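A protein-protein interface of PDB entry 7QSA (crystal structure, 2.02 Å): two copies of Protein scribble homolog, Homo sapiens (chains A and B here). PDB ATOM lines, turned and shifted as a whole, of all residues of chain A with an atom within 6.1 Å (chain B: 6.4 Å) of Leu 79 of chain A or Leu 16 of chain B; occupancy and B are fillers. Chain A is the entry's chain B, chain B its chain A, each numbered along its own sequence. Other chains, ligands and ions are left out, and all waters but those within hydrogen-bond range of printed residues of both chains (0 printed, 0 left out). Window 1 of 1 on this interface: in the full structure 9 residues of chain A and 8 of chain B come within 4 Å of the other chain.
CB of Ser 17 of chain B touches CG1 of Val 75 of chain A, 3.6 Å away. Lys 40 of chain B touches Ser 76 of chain A (CE to OG, 3.7 Å). Leu 79 of chain A touches Gly 15 of chain B (CD1 to C, 3.6 Å). CD1 of Leu 79 of chain A touches N of Leu 16 of chain B, at 3.6 Å. CD2 of Leu 79 of chain A touches OG of Ser 17 of chain B, 3.9995 Å away. CG of Lys 40 of chain B touches CD2 of Leu 79 of chain A, 3.6 Å away. CD2 of Leu 42 of chain B touches O of Leu 79 of chain A (3.6 Å). O of Arg 80 of chain A touches CD1 of Leu 42 of chain B, at 3.6 Å. Leu 42 of chain B touches Pro 81 of chain A.
Position printed for both chains: 78. Of the 9 pairs that touch across the chains among the printed residues, none has its exchanged pair printed and touching as well.
Of the printed residues of chain B, Ser 76 of chain A touches Lys 40 (3.7 Å). Printed residues of chain B within 4 Å of Leu 79 of chain A: Gly 15, Leu 16, Ser 17, Lys 40 and Leu 42. Of the printed residues of chain A, Gly 15 of chain B touches Leu 79 (3.6 Å). Printed residues of chain A within 4 Å of Leu 16 of chain B: Leu 79. Printed residues of chain A within 4 Å of Ser 17 of chain B: Val 75 and Leu 79. Of the printed residues of chain A, Lys 40 of chain B touches Ser 76 and Leu 79. Printed residues of chain A within 4 Å of Leu 42 of chain B: Leu 79, Arg 80 and Pro 81. The nearest printed residue of chain A that does not touch Leu 42 of chain B is Ser 76 of chain A (6.3 Å).
O of Gly 15 of chain B is in hydrogen-bond range of N of Leu 42 of chain B, at 2.8 Å. O of Ser 17 of chain B lies within hydrogen-bond range of N of Ser 39 of chain B (2.8 Å). N of Ser 17 of chain B sits at hydrogen-bond distance from O of Lys 40 of chain B (2.9 Å).
Of the 15 printed residues of chain B, 5 touch a printed residue of chain A. Hydrophobic or aromatic side chains of chain B that line the printed part of chain A: Leu 42. Along chain B the printed residues that touch a printed residue of chain A span positions 15 to 42. Among the printed residues, 9 pairs touch across the chains.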
ATOM      1  N   ALA A  74      21.892   2.593   5.187  1.00  0.00           N
ATOM      2  CA  ALA A  74      22.961   1.961   5.953  1.00  0.00           C
ATOM      3  C   ALA A  74      23.154   2.658   7.295  1.00  0.00           C
ATOM      4  O   ALA A  74      23.208   2.008   8.350  1.00  0.00           O
ATOM      5  CB  ALA A  74      24.247   1.971   5.138  1.00  0.00           C
ATOM      6  N   VAL A  75      23.213   3.993   7.272  1.00  0.00           N
ATOM      7  CA  VAL A  75      23.464   4.770   8.478  1.00  0.00           C
ATOM      8  C   VAL A  75      22.409   4.459   9.530  1.00  0.00           C
ATOM      9  O   VAL A  75      22.728   4.107  10.669  1.00  0.00           O
ATOM     10  CB  VAL A  75      23.481   6.264   8.113  1.00  0.00           C
ATOM     11  CG1 VAL A  75      23.602   7.130   9.316  1.00  0.00           C
ATOM     12  CG2 VAL A  75      24.618   6.551   7.136  1.00  0.00           C
ATOM     13  N   SER A  76      21.138   4.558   9.137  1.00  0.00           N
ATOM     14  CA  SER A  76      20.026   4.251  10.029  1.00  0.00           C
ATOM     15  C   SER A  76      20.124   2.841  10.573  1.00  0.00           C
ATOM     16  O   SER A  76      19.659   2.572  11.690  1.00  0.00           O
ATOM     17  CB  SER A  76      18.666   4.403   9.308  1.00  0.00           C
ATOM     18  OG  SER A  76      18.567   5.656   8.662  1.00  0.00           O
ATOM     19  N   ALA A  77      20.677   1.920   9.788  1.00  0.00           N
ATOM     20  CA  ALA A  77      20.832   0.567  10.315  1.00  0.00           C
ATOM     21  C   ALA A  77      21.979   0.502  11.295  1.00  0.00           C
ATOM     22  O   ALA A  77      21.932  -0.266  12.249  1.00  0.00           O
ATOM     23  CB  ALA A  77      21.104  -0.460   9.216  1.00  0.00           C
ATOM     24  N   LEU A  78      23.036   1.266  11.059  1.00  0.00           N
ATOM     25  CA  LEU A  78      24.120   1.257  12.027  1.00  0.00           C
ATOM     26  C   LEU A  78      23.728   2.019  13.281  1.00  0.00           C
ATOM     27  O   LEU A  78      24.199   1.710  14.373  1.00  0.00           O
ATOM     28  CB  LEU A  78      25.364   1.844  11.393  1.00  0.00           C
ATOM     29  CG  LEU A  78      25.858   0.893  10.312  1.00  0.00           C
ATOM     30  CD1 LEU A  78      26.768   1.576   9.309  1.00  0.00           C
ATOM     31  CD2 LEU A  78      26.517  -0.293  10.972  1.00  0.00           C
ATOM     32  N   LEU A  79      22.833   2.980  13.163  1.00  0.00           N
ATOM     33  CA  LEU A  79      22.513   3.831  14.289  1.00  0.00           C
ATOM     34  C   LEU A  79      21.393   3.163  15.065  1.00  0.00           C
ATOM     35  O   LEU A  79      20.214   3.465  14.864  1.00  0.00           O
ATOM     36  CB  LEU A  79      22.100   5.210  13.817  1.00  0.00           C
ATOM     37  CG  LEU A  79      21.745   6.227  14.892  1.00  0.00           C
ATOM     38  CD1 LEU A  79      22.885   6.531  15.816  1.00  0.00           C
ATOM     39  CD2 LEU A  79      21.294   7.485  14.112  1.00  0.00           C
ATOM     40  N   ARG A  80      21.757   2.267  15.965  1.00  0.00           N
ATOM     41  CA  ARG A  80      20.747   1.448  16.622  1.00  0.00           C
ATOM     42  C   ARG A  80      20.575   1.877  18.078  1.00  0.00           C
ATOM     43  O   ARG A  80      21.560   2.170  18.766  1.00  0.00           O
ATOM     44  CB  ARG A  80      21.109  -0.051  16.569  1.00  0.00           C
ATOM     45  CG  ARG A  80      21.170  -0.662  15.141  1.00  0.00           C
ATOM     46  CD  ARG A  80      19.844  -1.319  14.673  1.00  0.00           C
ATOM     47  NE  ARG A  80      18.758  -0.349  14.588  1.00  0.00           N
ATOM     48  CZ  ARG A  80      17.509  -0.591  14.958  1.00  0.00           C
ATOM     49  NH1 ARG A  80      17.130  -1.797  15.354  1.00  0.00           N
ATOM     50  NH2 ARG A  80      16.626   0.405  14.955  1.00  0.00           N
ATOM     51  N   PRO A  81      19.338   1.924  18.580  1.00  0.00           N
ATOM     52  CA  PRO A  81      19.222   2.210  20.023  1.00  0.00           C
ATOM     53  C   PRO A  81      20.014   1.197  20.872  1.00  0.00           C
ATOM     54  O   PRO A  81      20.597   1.669  21.865  1.00  0.00           O
ATOM     55  CB  PRO A  81      17.710   2.099  20.308  1.00  0.00           C
ATOM     56  CG  PRO A  81      17.024   1.979  18.959  1.00  0.00           C
ATOM     57  CD  PRO A  81      18.067   1.484  17.964  1.00  0.00           C
ATOM     58  N   LEU B   7      27.869  18.553  24.863  1.00  0.00           N
ATOM     59  CA  LEU B   7      27.687  17.200  24.378  1.00  0.00           C
ATOM     60  C   LEU B   7      28.624  16.274  25.150  1.00  0.00           C
ATOM     61  O   LEU B   7      29.840  16.538  25.203  1.00  0.00           O
ATOM     62  CB  LEU B   7      27.996  17.137  22.880  1.00  0.00           C
ATOM     63  CG  LEU B   7      27.925  15.778  22.190  1.00  0.00           C
ATOM     64  CD1 LEU B   7      26.474  15.341  21.954  1.00  0.00           C
ATOM     65  CD2 LEU B   7      28.699  15.745  20.865  1.00  0.00           C
ATOM     66  N   PRO B  13      27.107   4.965  23.745  1.00  0.00           N
ATOM     67  CA  PRO B  13      27.268   5.840  22.572  1.00  0.00           C
ATOM     68  C   PRO B  13      26.302   7.017  22.628  1.00  0.00           C
ATOM     69  O   PRO B  13      25.407   7.021  23.482  1.00  0.00           O
ATOM     70  CB  PRO B  13      26.980   4.904  21.386  1.00  0.00           C
ATOM     71  CG  PRO B  13      26.008   3.924  21.942  1.00  0.00           C
ATOM     72  CD  PRO B  13      26.362   3.733  23.403  1.00  0.00           C
ATOM     73  N   LEU B  14      26.503   7.989  21.728  1.00  0.00           N
ATOM     74  CA  LEU B  14      25.780   9.260  21.761  1.00  0.00           C
ATOM     75  C   LEU B  14      24.439   9.216  21.047  1.00  0.00           C
ATOM     76  O   LEU B  14      23.584  10.087  21.289  1.00  0.00           O
ATOM     77  CB  LEU B  14      26.581  10.383  21.087  1.00  0.00           C
ATOM     78  CG  LEU B  14      27.944  10.716  21.661  1.00  0.00           C
ATOM     79  CD1 LEU B  14      28.532  11.946  21.059  1.00  0.00           C
ATOM     80  CD2 LEU B  14      27.756  10.877  23.126  1.00  0.00           C
ATOM     81  N   GLY B  15      24.282   8.287  20.118  1.00  0.00           N
ATOM     82  CA  GLY B  15      23.063   8.172  19.356  1.00  0.00           C
ATOM     83  C   GLY B  15      22.923   9.212  18.274  1.00  0.00           C
ATOM     84  O   GLY B  15      21.822   9.765  18.115  1.00  0.00           O
ATOM     85  N   LEU B  16      24.013   9.504  17.539  1.00  0.00           N
ATOM     86  CA  LEU B  16      23.951  10.443  16.428  1.00  0.00           C
ATOM     87  C   LEU B  16      24.817   9.979  15.269  1.00  0.00           C
ATOM     88  O   LEU B  16      25.799   9.248  15.437  1.00  0.00           O
ATOM     89  CB  LEU B  16      24.431  11.879  16.777  1.00  0.00           C
ATOM     90  CG  LEU B  16      25.913  12.056  17.034  1.00  0.00           C
ATOM     91  CD1 LEU B  16      26.709  12.267  15.777  1.00  0.00           C
ATOM     92  CD2 LEU B  16      26.207  13.222  17.967  1.00  0.00           C
ATOM     93  N   SER B  17      24.482  10.468  14.082  1.00  0.00           N
ATOM     94  CA  SER B  17      25.341  10.322  12.921  1.00  0.00           C
ATOM     95  C   SER B  17      25.587  11.706  12.373  1.00  0.00           C
ATOM     96  O   SER B  17      24.714  12.573  12.454  1.00  0.00           O
ATOM     97  CB  SER B  17      24.686   9.448  11.838  1.00  0.00           C
ATOM     98  OG  SER B  17      23.338   9.873  11.639  1.00  0.00           O
ATOM     99  N   ILE B  18      26.780  11.919  11.852  1.00  0.00           N
ATOM    100  CA  ILE B  18      27.147  13.147  11.174  1.00  0.00           C
ATOM    101  C   ILE B  18      27.557  12.794   9.750  1.00  0.00           C
ATOM    102  O   ILE B  18      28.012  11.671   9.467  1.00  0.00           O
ATOM    103  CB  ILE B  18      28.281  13.900  11.897  1.00  0.00           C
ATOM    104  CG1 ILE B  18      29.572  13.094  11.913  1.00  0.00           C
ATOM    105  CG2 ILE B  18      27.937  14.186  13.407  1.00  0.00           C
ATOM    106  CD1 ILE B  18      30.800  13.943  12.141  1.00  0.00           C
ATOM    107  N   ILE B  38      24.762  17.196  11.451  1.00  0.00           N
ATOM    108  CA  ILE B  38      24.071  16.136  12.169  1.00  0.00           C
ATOM    109  C   ILE B  38      23.004  15.540  11.241  1.00  0.00           C
ATOM    110  O   ILE B  38      22.012  16.209  10.909  1.00  0.00           O
ATOM    111  CB  ILE B  38      23.453  16.680  13.452  1.00  0.00           C
ATOM    112  CG1 ILE B  38      24.496  17.413  14.338  1.00  0.00           C
ATOM    113  CG2 ILE B  38      22.822  15.574  14.300  1.00  0.00           C
ATOM    114  CD1 ILE B  38      25.524  16.535  14.897  1.00  0.00           C
ATOM    115  N   SER B  39      23.189  14.276  10.827  1.00  0.00           N
ATOM    116  CA  SER B  39      22.243  13.692   9.881  1.00  0.00           C
ATOM    117  C   SER B  39      21.158  12.856  10.559  1.00  0.00           C
ATOM    118  O   SER B  39      20.155  12.522   9.923  1.00  0.00           O
ATOM    119  CB  SER B  39      22.964  12.805   8.870  1.00  0.00           C
ATOM    120  OG  SER B  39      23.597  11.755   9.570  1.00  0.00           O
ATOM    121  N   LYS B  40      21.342  12.463  11.807  1.00  0.00           N
ATOM    122  CA  LYS B  40      20.292  11.706  12.458  1.00  0.00           C
ATOM    123  C   LYS B  40      20.613  11.636  13.943  1.00  0.00           C
ATOM    124  O   LYS B  40      21.792  11.503  14.324  1.00  0.00           O
ATOM    125  CB  LYS B  40      20.191  10.317  11.838  1.00  0.00           C
ATOM    126  CG  LYS B  40      18.942   9.516  12.301  1.00  0.00           C
ATOM    127  CD  LYS B  40      18.782   8.223  11.483  1.00  0.00           C
ATOM    128  CE  LYS B  40      17.429   7.516  11.705  1.00  0.00           C
ATOM    129  NZ  LYS B  40      17.339   6.822  13.026  1.00  0.00           N
ATOM    130  N   VAL B  41      19.579  11.715  14.770  1.00  0.00           N
ATOM    131  CA  VAL B  41      19.719  11.578  16.209  1.00  0.00           C
ATOM    132  C   VAL B  41      18.646  10.609  16.696  1.00  0.00           C
ATOM    133  O   VAL B  41      17.462  10.721  16.324  1.00  0.00           O
ATOM    134  CB  VAL B  41      19.613  12.935  16.927  1.00  0.00           C
ATOM    135  CG1 VAL B  41      19.625  12.730  18.406  1.00  0.00           C
ATOM    136  CG2 VAL B  41      20.817  13.816  16.557  1.00  0.00           C
ATOM    137  N   LEU B  42      19.058   9.661  17.522  1.00  0.00           N
ATOM    138  CA  LEU B  42      18.097   8.758  18.133  1.00  0.00           C
ATOM    139  C   LEU B  42      17.285   9.527  19.171  1.00  0.00           C
ATOM    140  O   LEU B  42      17.854  10.267  19.984  1.00  0.00           O
ATOM    141  CB  LEU B  42      18.798   7.570  18.786  1.00  0.00           C
ATOM    142  CG  LEU B  42      19.538   6.635  17.837  1.00  0.00           C
ATOM    143  CD1 LEU B  42      20.223   5.510  18.639  1.00  0.00           C
ATOM    144  CD2 LEU B  42      18.621   6.005  16.814  1.00  0.00           C
ATOM    145  N   ALA B  47      22.733  12.495  22.388  1.00  0.00           N
ATOM    146  CA  ALA B  47      22.824  13.680  21.535  1.00  0.00           C
ATOM    147  C   ALA B  47      21.520  14.456  21.571  1.00  0.00           C
ATOM    148  O   ALA B  47      21.496  15.685  21.736  1.00  0.00           O
ATOM    149  CB  ALA B  47      23.154  13.259  20.095  1.00  0.00           C
ATOM    150  N   LEU B  52      21.161  18.712  20.495  1.00  0.00           N
ATOM    151  CA  LEU B  52      21.513  18.667  19.094  1.00  0.00           C
ATOM    152  C   LEU B  52      20.304  18.255  18.271  1.00  0.00           C
ATOM    153  O   LEU B  52      19.431  17.496  18.728  1.00  0.00           O
ATOM    154  CB  LEU B  52      22.624  17.662  18.825  1.00  0.00           C
ATOM    155  CG  LEU B  52      24.045  18.107  19.069  1.00  0.00           C
ATOM    156  CD1 LEU B  52      24.935  16.948  18.596  1.00  0.00           C
ATOM    157  CD2 LEU B  52      24.439  19.352  18.297  1.00  0.00           C
ATOM    158  N   LEU B  78      35.344  15.359  17.641  1.00  0.00           N
ATOM    159  CA  LEU B  78      34.224  14.973  18.474  1.00  0.00           C
ATOM    160  C   LEU B  78      34.583  13.789  19.334  1.00  0.00           C
ATOM    161  O   LEU B  78      33.846  13.473  20.279  1.00  0.00           O
ATOM    162  CB  LEU B  78      33.023  14.582  17.603  1.00  0.00           C
ATOM    163  CG  LEU B  78      32.271  15.681  16.841  1.00  0.00           C
ATOM    164  CD1 LEU B  78      31.285  15.046  15.842  1.00  0.00           C
ATOM    165  CD2 LEU B  78      31.579  16.586  17.831  1.00  0.00           C
